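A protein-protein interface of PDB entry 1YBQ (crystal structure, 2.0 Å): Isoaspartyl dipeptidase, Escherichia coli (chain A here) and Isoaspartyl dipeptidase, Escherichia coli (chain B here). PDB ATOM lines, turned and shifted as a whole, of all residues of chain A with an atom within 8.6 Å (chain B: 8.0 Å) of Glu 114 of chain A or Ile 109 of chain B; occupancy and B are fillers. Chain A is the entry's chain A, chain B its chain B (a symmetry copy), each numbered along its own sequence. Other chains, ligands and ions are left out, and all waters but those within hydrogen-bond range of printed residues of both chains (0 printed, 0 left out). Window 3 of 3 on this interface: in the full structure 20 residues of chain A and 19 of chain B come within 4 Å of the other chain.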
ATOM      1  N   ILE A  72      16.592   3.554  15.653  1.00  0.00           N
ATOM      2  CA  ILE A  72      16.193   4.113  14.355  1.00  0.00           C
ATOM      3  C   ILE A  72      16.532   3.239  13.182  1.00  0.00           C
ATOM      4  O   ILE A  72      16.259   3.595  12.041  1.00  0.00           O
ATOM      5  CB  ILE A  72      16.721   5.541  14.069  1.00  0.00           C
ATOM      6  CG1 ILE A  72      18.255   5.608  13.955  1.00  0.00           C
ATOM      7  CG2 ILE A  72      16.179   6.531  15.091  1.00  0.00           C
ATOM      8  CD1 ILE A  72      18.813   6.999  13.706  1.00  0.00           C
ATOM      9  N   LEU A 104      23.837   4.309  17.604  1.00  0.00           N
ATOM     10  CA  LEU A 104      24.131   4.182  16.166  1.00  0.00           C
ATOM     11  C   LEU A 104      25.353   3.238  16.024  1.00  0.00           C
ATOM     12  O   LEU A 104      26.068   3.007  17.030  1.00  0.00           O
ATOM     13  CB  LEU A 104      24.410   5.535  15.466  1.00  0.00           C
ATOM     14  CG  LEU A 104      23.305   6.605  15.533  1.00  0.00           C
ATOM     15  CD1 LEU A 104      23.816   7.830  14.766  1.00  0.00           C
ATOM     16  CD2 LEU A 104      21.951   6.117  15.001  1.00  0.00           C
ATOM     17  N   SER A 108      27.083   6.280  10.041  1.00  0.00           N
ATOM     18  CA  SER A 108      26.768   7.556  10.613  1.00  0.00           C
ATOM     19  C   SER A 108      26.727   8.596   9.502  1.00  0.00           C
ATOM     20  O   SER A 108      27.045   9.761   9.722  1.00  0.00           O
ATOM     21  CB  SER A 108      27.598   7.974  11.832  1.00  0.00           C
ATOM     22  OG  SER A 108      28.978   7.892  11.567  1.00  0.00           O
ATOM     23  N   ARG A 111      22.610   7.929   8.863  1.00  0.00           N
ATOM     24  CA  ARG A 111      22.049   7.846  10.252  1.00  0.00           C
ATOM     25  C   ARG A 111      22.574   9.026  11.070  1.00  0.00           C
ATOM     26  O   ARG A 111      23.768   9.307  11.009  1.00  0.00           O
ATOM     27  CB  ARG A 111      22.359   6.553  11.016  1.00  0.00           C
ATOM     28  CG  ARG A 111      21.946   5.275  10.311  1.00  0.00           C
ATOM     29  CD  ARG A 111      20.464   5.187   9.948  1.00  0.00           C
ATOM     30  NE  ARG A 111      20.098   3.828   9.535  1.00  0.00           N
ATOM     31  CZ  ARG A 111      18.844   3.420   9.358  1.00  0.00           C
ATOM     32  NH1 ARG A 111      17.781   4.209   9.536  1.00  0.00           N
ATOM     33  NH2 ARG A 111      18.650   2.163   8.996  1.00  0.00           N
ATOM     34  N   HIS A 112      21.675   9.694  11.820  1.00  0.00           N
ATOM     35  CA  HIS A 112      21.993  10.921  12.548  1.00  0.00           C
ATOM     36  C   HIS A 112      21.547  10.957  14.004  1.00  0.00           C
ATOM     37  O   HIS A 112      20.467  10.478  14.318  1.00  0.00           O
ATOM     38  CB  HIS A 112      21.343  12.114  11.772  1.00  0.00           C
ATOM     39  CG  HIS A 112      21.622  12.064  10.293  1.00  0.00           C
ATOM     40  ND1 HIS A 112      22.522  12.934   9.656  1.00  0.00           N
ATOM     41  CD2 HIS A 112      21.176  11.201   9.350  1.00  0.00           C
ATOM     42  CE1 HIS A 112      22.575  12.602   8.362  1.00  0.00           C
ATOM     43  NE2 HIS A 112      21.765  11.567   8.141  1.00  0.00           N
ATOM     44  N   PRO A 113      22.378  11.566  14.880  1.00  0.00           N
ATOM     45  CA  PRO A 113      22.030  11.642  16.273  1.00  0.00           C
ATOM     46  C   PRO A 113      20.749  12.427  16.454  1.00  0.00           C
ATOM     47  O   PRO A 113      19.979  12.118  17.333  1.00  0.00           O
ATOM     48  CB  PRO A 113      23.188  12.298  17.010  1.00  0.00           C
ATOM     49  CG  PRO A 113      24.300  12.475  16.010  1.00  0.00           C
ATOM     50  CD  PRO A 113      23.725  12.132  14.651  1.00  0.00           C
ATOM     51  N   GLU A 114      20.482  13.421  15.611  1.00  0.00           N
ATOM     52  CA  GLU A 114      19.229  14.147  15.775  1.00  0.00           C
ATOM     53  C   GLU A 114      18.046  13.248  15.544  1.00  0.00           C
ATOM     54  O   GLU A 114      16.991  13.414  16.157  1.00  0.00           O
ATOM     55  CB  GLU A 114      19.084  15.294  14.786  1.00  0.00           C
ATOM     56  CG  GLU A 114      20.115  16.351  15.112  1.00  0.00           C
ATOM     57  CD  GLU A 114      21.462  15.983  14.581  1.00  0.00           C
ATOM     58  OE1 GLU A 114      21.735  14.908  14.063  1.00  0.00           O
ATOM     59  OE2 GLU A 114      22.299  16.982  14.724  1.00  0.00           O
ATOM     60  N   SER A 115      18.182  12.303  14.635  1.00  0.00           N
ATOM     61  CA  SER A 115      17.040  11.428  14.395  1.00  0.00           C
ATOM     62  C   SER A 115      16.859  10.475  15.580  1.00  0.00           C
ATOM     63  O   SER A 115      15.756  10.268  16.064  1.00  0.00           O
ATOM     64  CB  SER A 115      17.163  10.668  13.075  1.00  0.00           C
ATOM     65  OG  SER A 115      17.744  11.466  12.061  1.00  0.00           O
ATOM     66  N   LEU A 116      17.983   9.908  16.054  1.00  0.00           N
ATOM     67  CA  LEU A 116      18.021   9.001  17.182  1.00  0.00           C
ATOM     68  C   LEU A 116      17.390   9.698  18.385  1.00  0.00           C
ATOM     69  O   LEU A 116      16.550   9.153  19.138  1.00  0.00           O
ATOM     70  CB  LEU A 116      19.477   8.527  17.461  1.00  0.00           C
ATOM     71  CG  LEU A 116      19.571   7.592  18.685  1.00  0.00           C
ATOM     72  CD1 LEU A 116      18.624   6.389  18.625  1.00  0.00           C
ATOM     73  CD2 LEU A 116      20.973   7.036  18.806  1.00  0.00           C
ATOM     74  N   LEU A 117      17.757  10.967  18.573  1.00  0.00           N
ATOM     75  CA  LEU A 117      17.210  11.719  19.691  1.00  0.00           C
ATOM     76  C   LEU A 117      15.697  11.867  19.576  1.00  0.00           C
ATOM     77  O   LEU A 117      14.980  11.740  20.567  1.00  0.00           O
ATOM     78  CB  LEU A 117      17.893  13.082  19.897  1.00  0.00           C
ATOM     79  CG  LEU A 117      17.231  13.998  20.941  1.00  0.00           C
ATOM     80  CD1 LEU A 117      17.572  13.599  22.385  1.00  0.00           C
ATOM     81  CD2 LEU A 117      17.724  15.415  20.703  1.00  0.00           C
ATOM     82  N   ALA A 118      15.185  12.120  18.377  1.00  0.00           N
ATOM     83  CA  ALA A 118      13.727  12.259  18.228  1.00  0.00           C
ATOM     84  C   ALA A 118      12.978  10.960  18.564  1.00  0.00           C
ATOM     85  O   ALA A 118      11.906  10.921  19.189  1.00  0.00           O
ATOM     86  CB  ALA A 118      13.409  12.724  16.801  1.00  0.00           C
ATOM     87  N   LYS A 119      13.571   9.851  18.107  1.00  0.00           N
ATOM     88  CA  LYS A 119      12.999   8.545  18.334  1.00  0.00           C
ATOM     89  C   LYS A 119      12.969   8.205  19.833  1.00  0.00           C
ATOM     90  O   LYS A 119      11.987   7.587  20.327  1.00  0.00           O
ATOM     91  CB  LYS A 119      13.746   7.469  17.522  1.00  0.00           C
ATOM     92  CG  LYS A 119      13.282   6.027  17.798  1.00  0.00           C
ATOM     93  CD  LYS A 119      11.909   5.716  17.224  1.00  0.00           C
ATOM     94  CE  LYS A 119      11.517   4.248  17.280  1.00  0.00           C
ATOM     95  NZ  LYS A 119      10.195   4.033  16.683  1.00  0.00           N
ATOM     96  N   THR A 120      14.066   8.593  20.530  1.00  0.00           N
ATOM     97  CA  THR A 120      14.219   8.375  21.978  1.00  0.00           C
ATOM     98  C   THR A 120      13.093   9.069  22.717  1.00  0.00           C
ATOM     99  O   THR A 120      12.471   8.521  23.615  1.00  0.00           O
ATOM    100  CB  THR A 120      15.604   8.782  22.504  1.00  0.00           C
ATOM    101  OG1 THR A 120      16.576   7.945  21.914  1.00  0.00           O
ATOM    102  CG2 THR A 120      15.630   8.512  23.990  1.00  0.00           C
ATOM    103  N   ARG A 121      12.791  10.280  22.276  1.00  0.00           N
ATOM    104  CA  ARG A 121      11.731  11.064  22.865  1.00  0.00           C
ATOM    105  C   ARG A 121      10.364  10.501  22.603  1.00  0.00           C
ATOM    106  O   ARG A 121       9.511  10.524  23.482  1.00  0.00           O
ATOM    107  CB  ARG A 121      11.821  12.535  22.494  1.00  0.00           C
ATOM    108  CG  ARG A 121      13.132  13.108  23.064  1.00  0.00           C
ATOM    109  CD  ARG A 121      13.331  14.620  22.897  1.00  0.00           C
ATOM    110  NE  ARG A 121      14.293  15.218  23.844  1.00  0.00           N
ATOM    111  CZ  ARG A 121      14.970  16.336  23.591  1.00  0.00           C
ATOM    112  NH1 ARG A 121      14.825  17.008  22.438  1.00  0.00           N
ATOM    113  NH2 ARG A 121      15.792  16.822  24.515  1.00  0.00           N
ATOM    114  N   MET A 132      19.972   7.650  25.081  1.00  0.00           N
ATOM    115  CA  MET A 132      20.816   7.400  23.940  1.00  0.00           C
ATOM    116  C   MET A 132      22.268   7.754  24.218  1.00  0.00           C
ATOM    117  O   MET A 132      22.569   8.465  25.184  1.00  0.00           O
ATOM    118  CB  MET A 132      20.343   8.189  22.701  1.00  0.00           C
ATOM    119  CG  MET A 132      20.562   9.695  22.833  1.00  0.00           C
ATOM    120  SD  MET A 132      20.028  10.604  21.361  1.00  0.00           S
ATOM    121  CE  MET A 132      21.606  10.594  20.472  1.00  0.00           C
ATOM    122  N   LEU A 133      23.126   7.239  23.332  1.00  0.00           N
ATOM    123  CA  LEU A 133      24.549   7.526  23.358  1.00  0.00           C
ATOM    124  C   LEU A 133      24.766   8.410  22.161  1.00  0.00           C
ATOM    125  O   LEU A 133      24.144   8.187  21.135  1.00  0.00           O
ATOM    126  CB  LEU A 133      25.416   6.273  23.057  1.00  0.00           C
ATOM    127  CG  LEU A 133      25.293   5.207  24.131  1.00  0.00           C
ATOM    128  CD1 LEU A 133      26.418   4.195  23.992  1.00  0.00           C
ATOM    129  CD2 LEU A 133      25.433   5.904  25.473  1.00  0.00           C
ATOM    130  N   THR A 134      25.651   9.367  22.259  1.00  0.00           N
ATOM    131  CA  THR A 134      25.991  10.163  21.115  1.00  0.00           C
ATOM    132  C   THR A 134      27.159   9.433  20.400  1.00  0.00           C
ATOM    133  O   THR A 134      27.688   8.414  20.875  1.00  0.00           O
ATOM    134  CB  THR A 134      26.390  11.599  21.522  1.00  0.00           C
ATOM    135  OG1 THR A 134      26.440  12.409  20.372  1.00  0.00           O
ATOM    136  CG2 THR A 134      27.745  11.615  22.252  1.00  0.00           C
ATOM    137  N   ARG A 142      30.628  11.895  15.732  1.00  0.00           N
ATOM    138  CA  ARG A 142      29.722  12.783  15.032  1.00  0.00           C
ATOM    139  C   ARG A 142      28.639  13.070  16.048  1.00  0.00           C
ATOM    140  O   ARG A 142      27.931  12.165  16.453  1.00  0.00           O
ATOM    141  CB  ARG A 142      29.174  12.092  13.813  1.00  0.00           C
ATOM    142  CG  ARG A 142      30.335  11.684  12.927  1.00  0.00           C
ATOM    143  CD  ARG A 142      29.914  11.652  11.481  1.00  0.00           C
ATOM    144  NE  ARG A 142      31.030  11.437  10.576  1.00  0.00           N
ATOM    145  CZ  ARG A 142      31.330  10.279   9.989  1.00  0.00           C
ATOM    146  NH1 ARG A 142      30.643   9.154  10.157  1.00  0.00           N
ATOM    147  NH2 ARG A 142      32.357  10.228   9.172  1.00  0.00           N
ATOM    148  N   THR A 143      28.568  14.295  16.514  1.00  0.00           N
ATOM    149  CA  THR A 143      27.658  14.695  17.572  1.00  0.00           C
ATOM    150  C   THR A 143      26.575  15.657  17.133  1.00  0.00           C
ATOM    151  O   THR A 143      26.481  16.025  15.981  1.00  0.00           O
ATOM    152  CB  THR A 143      28.487  15.395  18.646  1.00  0.00           C
ATOM    153  OG1 THR A 143      28.966  16.577  18.052  1.00  0.00           O
ATOM    154  CG2 THR A 143      29.691  14.540  19.044  1.00  0.00           C
ATOM    155  N   ILE A 144      25.772  16.088  18.083  1.00  0.00           N
ATOM    156  CA  ILE A 144      24.713  17.023  17.792  1.00  0.00           C
ATOM    157  C   ILE A 144      25.121  18.474  17.923  1.00  0.00           C
ATOM    158  O   ILE A 144      24.709  19.320  17.110  1.00  0.00           O
ATOM    159  CB  ILE A 144      23.566  16.810  18.761  1.00  0.00           C
ATOM    160  CG1 ILE A 144      22.956  15.465  18.482  1.00  0.00           C
ATOM    161  CG2 ILE A 144      22.510  17.892  18.569  1.00  0.00           C
ATOM    162  CD1 ILE A 144      22.489  14.765  19.749  1.00  0.00           C
ATOM    163  N   THR A 145      25.883  18.774  18.987  1.00  0.00           N
ATOM    164  CA  THR A 145      26.309  20.166  19.259  1.00  0.00           C
ATOM    165  C   THR A 145      27.705  20.487  18.760  1.00  0.00           C
ATOM    166  O   THR A 145      28.140  21.633  18.852  1.00  0.00           O
ATOM    167  CB  THR A 145      26.348  20.469  20.758  1.00  0.00           C
ATOM    168  OG1 THR A 145      27.287  19.574  21.348  1.00  0.00           O
ATOM    169  CG2 THR A 145      24.968  20.331  21.376  1.00  0.00           C
ATOM    170  N   GLY A 146      28.407  19.464  18.276  1.00  0.00           N
ATOM    171  CA  GLY A 146      29.758  19.646  17.805  1.00  0.00           C
ATOM    172  C   GLY A 146      30.786  19.183  18.837  1.00  0.00           C
ATOM    173  O   GLY A 146      31.977  19.060  18.554  1.00  0.00           O
ATOM    174  N   ASP A 151      27.446  17.585  24.221  1.00  0.00           N
ATOM    175  CA  ASP A 151      26.264  16.708  24.002  1.00  0.00           C
ATOM    176  C   ASP A 151      25.819  15.990  25.305  1.00  0.00           C
ATOM    177  O   ASP A 151      24.637  15.965  25.696  1.00  0.00           O
ATOM    178  CB  ASP A 151      26.467  15.639  22.884  1.00  0.00           C
ATOM    179  CG  ASP A 151      26.251  16.065  21.441  1.00  0.00           C
ATOM    180  OD1 ASP A 151      26.276  17.215  21.042  1.00  0.00           O
ATOM    181  OD2 ASP A 151      26.063  15.040  20.646  1.00  0.00           O
ATOM    182  N   ILE A 155      22.481  17.633  26.293  1.00  0.00           N
ATOM    183  CA  ILE A 155      21.260  17.066  25.717  1.00  0.00           C
ATOM    184  C   ILE A 155      20.724  16.116  26.751  1.00  0.00           C
ATOM    185  O   ILE A 155      21.408  15.146  27.138  1.00  0.00           O
ATOM    186  CB  ILE A 155      21.459  16.391  24.367  1.00  0.00           C
ATOM    187  CG1 ILE A 155      22.095  17.365  23.384  1.00  0.00           C
ATOM    188  CG2 ILE A 155      20.137  15.869  23.813  1.00  0.00           C
ATOM    189  CD1 ILE A 155      21.155  18.517  23.062  1.00  0.00           C
ATOM    190  N   VAL A 158      21.039  12.328  26.284  1.00  0.00           N
ATOM    191  CA  VAL A 158      22.353  11.736  26.064  1.00  0.00           C
ATOM    192  C   VAL A 158      23.030  11.365  27.360  1.00  0.00           C
ATOM    193  O   VAL A 158      23.157  12.240  28.201  1.00  0.00           O
ATOM    194  CB  VAL A 158      23.282  12.628  25.246  1.00  0.00           C
ATOM    195  CG1 VAL A 158      24.638  11.934  25.073  1.00  0.00           C
ATOM    196  CG2 VAL A 158      22.624  12.846  23.883  1.00  0.00           C
ATOM    197  N   ARG B  83       6.125  11.010  13.902  1.00  0.00           N
ATOM    198  CA  ARG B  83       7.036  10.856  12.777  1.00  0.00           C
ATOM    199  C   ARG B  83       6.616   9.564  12.075  1.00  0.00           C
ATOM    200  O   ARG B  83       6.688   8.477  12.678  1.00  0.00           O
ATOM    201  CB  ARG B  83       8.474  10.696  13.246  1.00  0.00           C
ATOM    202  CG  ARG B  83       8.926  12.052  13.761  1.00  0.00           C
ATOM    203  CD  ARG B  83      10.177  11.877  14.574  1.00  0.00           C
ATOM    204  NE  ARG B  83      11.345  11.751  13.715  1.00  0.00           N
ATOM    205  CZ  ARG B  83      12.064  10.635  13.532  1.00  0.00           C
ATOM    206  NH1 ARG B  83      11.762   9.478  14.130  1.00  0.00           N
ATOM    207  NH2 ARG B  83      13.124  10.672  12.731  1.00  0.00           N
ATOM    208  N   LEU B 104      11.270  15.686   1.414  1.00  0.00           N
ATOM    209  CA  LEU B 104      11.090  15.970   2.826  1.00  0.00           C
ATOM    210  C   LEU B 104       9.974  16.994   2.942  1.00  0.00           C
ATOM    211  O   LEU B 104       9.601  17.639   1.943  1.00  0.00           O
ATOM    212  CB  LEU B 104      12.364  16.433   3.556  1.00  0.00           C
ATOM    213  CG  LEU B 104      13.541  15.457   3.402  1.00  0.00           C
ATOM    214  CD1 LEU B 104      14.723  16.042   4.146  1.00  0.00           C
ATOM    215  CD2 LEU B 104      13.204  14.083   3.958  1.00  0.00           C
ATOM    216  N   GLY B 105       9.414  17.096   4.132  1.00  0.00           N
ATOM    217  CA  GLY B 105       8.322  18.005   4.361  1.00  0.00           C
ATOM    218  C   GLY B 105       8.664  18.943   5.476  1.00  0.00           C
ATOM    219  O   GLY B 105       9.709  19.575   5.487  1.00  0.00           O
ATOM    220  N   THR B 106       7.754  19.028   6.416  1.00  0.00           N
ATOM    221  CA  THR B 106       7.925  19.917   7.540  1.00  0.00           C
ATOM    222  C   THR B 106       9.214  19.734   8.333  1.00  0.00           C
ATOM    223  O   THR B 106       9.899  20.677   8.703  1.00  0.00           O
ATOM    224  CB  THR B 106       6.735  19.799   8.511  1.00  0.00           C
ATOM    225  OG1 THR B 106       5.521  19.873   7.779  1.00  0.00           O
ATOM    226  CG2 THR B 106       6.801  20.952   9.510  1.00  0.00           C
ATOM    227  N   ASP B 107       9.534  18.507   8.659  1.00  0.00           N
ATOM    228  CA  ASP B 107      10.707  18.265   9.469  1.00  0.00           C
ATOM    229  C   ASP B 107      11.974  18.022   8.664  1.00  0.00           C
ATOM    230  O   ASP B 107      12.098  17.065   7.893  1.00  0.00           O
ATOM    231  CB  ASP B 107      10.383  17.072  10.393  1.00  0.00           C
ATOM    232  CG  ASP B 107      11.530  16.652  11.279  1.00  0.00           C
ATOM    233  OD1 ASP B 107      12.595  17.207  11.350  1.00  0.00           O
ATOM    234  OD2 ASP B 107      11.266  15.571  11.941  1.00  0.00           O
ATOM    235  N   SER B 108      12.945  18.892   8.883  1.00  0.00           N
ATOM    236  CA  SER B 108      14.262  18.767   8.259  1.00  0.00           C
ATOM    237  C   SER B 108      15.347  18.860   9.352  1.00  0.00           C
ATOM    238  O   SER B 108      16.485  19.288   9.107  1.00  0.00           O
ATOM    239  CB  SER B 108      14.513  19.670   7.033  1.00  0.00           C
ATOM    240  OG  SER B 108      14.408  21.057   7.354  1.00  0.00           O
ATOM    241  N   ILE B 109      14.934  18.508  10.587  1.00  0.00           N
ATOM    242  CA  ILE B 109      15.798  18.464  11.754  1.00  0.00           C
ATOM    243  C   ILE B 109      16.130  17.005  12.116  1.00  0.00           C
ATOM    244  O   ILE B 109      17.286  16.628  12.419  1.00  0.00           O
ATOM    245  CB  ILE B 109      15.143  19.059  12.980  1.00  0.00           C
ATOM    246  CG1 ILE B 109      14.683  20.487  12.736  1.00  0.00           C
ATOM    247  CG2 ILE B 109      16.097  18.939  14.164  1.00  0.00           C
ATOM    248  CD1 ILE B 109      15.733  21.531  13.060  1.00  0.00           C
ATOM    249  N   SER B 110      15.076  16.186  12.126  1.00  0.00           N
ATOM    250  CA  SER B 110      15.247  14.784  12.445  1.00  0.00           C
ATOM    251  C   SER B 110      15.254  14.011  11.147  1.00  0.00           C
ATOM    252  O   SER B 110      15.408  12.790  11.163  1.00  0.00           O
ATOM    253  CB  SER B 110      14.135  14.274  13.343  1.00  0.00           C
ATOM    254  OG  SER B 110      13.010  14.000  12.519  1.00  0.00           O
ATOM    255  N   ARG B 111      15.048  14.746  10.029  1.00  0.00           N
ATOM    256  CA  ARG B 111      15.014  14.185   8.653  1.00  0.00           C
ATOM    257  C   ARG B 111      16.147  14.818   7.862  1.00  0.00           C
ATOM    258  O   ARG B 111      16.307  16.038   7.922  1.00  0.00           O
ATOM    259  CB  ARG B 111      13.692  14.409   7.911  1.00  0.00           C
ATOM    260  CG  ARG B 111      12.456  13.869   8.646  1.00  0.00           C
ATOM    261  CD  ARG B 111      12.570  12.396   9.111  1.00  0.00           C
ATOM    262  NE  ARG B 111      11.233  11.862   9.482  1.00  0.00           N
ATOM    263  CZ  ARG B 111      10.890  10.585   9.651  1.00  0.00           C
ATOM    264  NH1 ARG B 111      11.775   9.587   9.533  1.00  0.00           N
ATOM    265  NH2 ARG B 111       9.616  10.309   9.962  1.00  0.00           N
ATOM    266  N   HIS B 112      16.908  13.992   7.137  1.00  0.00           N
ATOM    267  CA  HIS B 112      18.083  14.433   6.386  1.00  0.00           C
ATOM    268  C   HIS B 112      18.161  13.973   4.927  1.00  0.00           C
ATOM    269  O   HIS B 112      17.874  12.817   4.642  1.00  0.00           O
ATOM    270  CB  HIS B 112      19.346  13.930   7.148  1.00  0.00           C
ATOM    271  CG  HIS B 112      19.276  14.228   8.608  1.00  0.00           C
ATOM    272  ND1 HIS B 112      18.551  13.421   9.478  1.00  0.00           N
ATOM    273  CD2 HIS B 112      19.805  15.251   9.326  1.00  0.00           C
ATOM    274  CE1 HIS B 112      18.663  13.940  10.703  1.00  0.00           C
ATOM    275  NE2 HIS B 112      19.400  15.040  10.645  1.00  0.00           N
ATOM    276  N   ALA B 136      13.589  20.985   1.692  1.00  0.00           N
ATOM    277  CA  ALA B 136      12.442  20.615   2.519  1.00  0.00           C
ATOM    278  C   ALA B 136      11.553  21.842   2.600  1.00  0.00           C
ATOM    279  O   ALA B 136      11.638  22.739   1.777  1.00  0.00           O
ATOM    280  CB  ALA B 136      12.901  20.250   3.932  1.00  0.00           C
ATOM    281  N   HIS B 138      11.797  24.178   4.726  1.00  0.00           N
ATOM    282  CA  HIS B 138      12.757  25.189   5.154  1.00  0.00           C
ATOM    283  C   HIS B 138      13.486  25.858   4.033  1.00  0.00           C
ATOM    284  O   HIS B 138      14.101  25.211   3.164  1.00  0.00           O
ATOM    285  CB  HIS B 138      13.810  24.690   6.176  1.00  0.00           C
ATOM    286  CG  HIS B 138      14.466  25.857   6.864  1.00  0.00           C
ATOM    287  ND1 HIS B 138      15.566  26.488   6.314  1.00  0.00           N
ATOM    288  CD2 HIS B 138      14.131  26.532   8.019  1.00  0.00           C
ATOM    289  CE1 HIS B 138      15.889  27.489   7.140  1.00  0.00           C
ATOM    290  NE2 HIS B 138      15.047  27.545   8.165  1.00  0.00           N
ATOM    291  N   ARG B 142      18.230  23.103   3.270  1.00  0.00           N
ATOM    292  CA  ARG B 142      19.252  22.328   3.919  1.00  0.00           C
ATOM    293  C   ARG B 142      19.631  21.290   2.853  1.00  0.00           C
ATOM    294  O   ARG B 142      18.742  20.618   2.315  1.00  0.00           O
ATOM    295  CB  ARG B 142      18.802  21.762   5.244  1.00  0.00           C
ATOM    296  CG  ARG B 142      18.101  22.805   6.101  1.00  0.00           C
ATOM    297  CD  ARG B 142      17.857  22.262   7.494  1.00  0.00           C
ATOM    298  NE  ARG B 142      17.661  23.338   8.448  1.00  0.00           N
ATOM    299  CZ  ARG B 142      16.519  23.589   9.067  1.00  0.00           C
ATOM    300  NH1 ARG B 142      15.399  22.864   8.900  1.00  0.00           N
ATOM    301  NH2 ARG B 142      16.506  24.618   9.898  1.00  0.00           N
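OD2 of Asp 107 of chain B is in hydrogen-bond range of OG of Ser 110 of chain B.
The backbone carbonyl oxygen (O) of Ile 109 of chain B sits at hydrogen-bond distance from a ring nitrogen (NE2) of His 112 of chain B, at 3.2 Å.
The guanidinium group of Arg 83 of chain B lies within hydrogen-bond range of the side-chain hydroxyl of Ser 110 of chain B, at 3.0 Å.
N of Ile 109 of chain B is in hydrogen-bond range of OD1 of Asp 107 of chain B (2.8 Å).
Among the printed residues, 6 pairs touch across the chains.
Among the printed residues, no Asp or Glu carboxylate lies within 4 Å of a Lys or Arg side-chain nitrogen of the other chain.
OG of Ser 115 of chain A lies close to ND1 of His 112 of chain B (3.3 Å).
OG of Ser 115 of chain A lies within hydrogen-bond range of O of Ser 110 of chain B, at 2.8 Å.
Among the printed residues, pairs that only touch across the chains: Glu 114 of chain A with Ile 109 of chain B (3.3 Å), His 112 of chain A with His 112 of chain B (3.4 Å), Ala 118 of chain A with Arg 83 of chain B (3.8 Å) and Ala 118 of chain A with Ser 110 of chain B (3.9 Å).
Of chain B, only Ile 109 comes within 4 Å of Glu 114 of chain A.
Of chain A, only Glu 114 (3.3 Å) comes within 4 Å of Ile 109 of chain B.
Of chain B, only Ser 110 (2.8 Å) and His 112 (3.0 Å) come within 4 Å of Ser 115 of chain A.
No residue of chain A comes within 4 Å of Ser 108 of chain B.
Of the printed residues of chain B, His 112 of chain A touches His 112.
Printed residues of chain A within 4 Å of His 112 of chain B: His 112 and Ser 115.
Of the printed residues of chain B, Ala 118 of chain A touches Arg 83 and Ser 110.
Of the printed residues of chain A, Arg 83 of chain B touches Ala 118 (3.8 Å).
Leu 117 of chain A touches none of the printed residues of chain B.
His 138 of chain B touches none of the printed residues of chain A.
The nearest residue of chain B that does not touch Glu 114 of chain A is Ser 110 of chain B (4.1 Å).
The nearest printed residue of chain B that does not touch His 112 of chain A is Ser 110 of chain B (6.0 Å).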
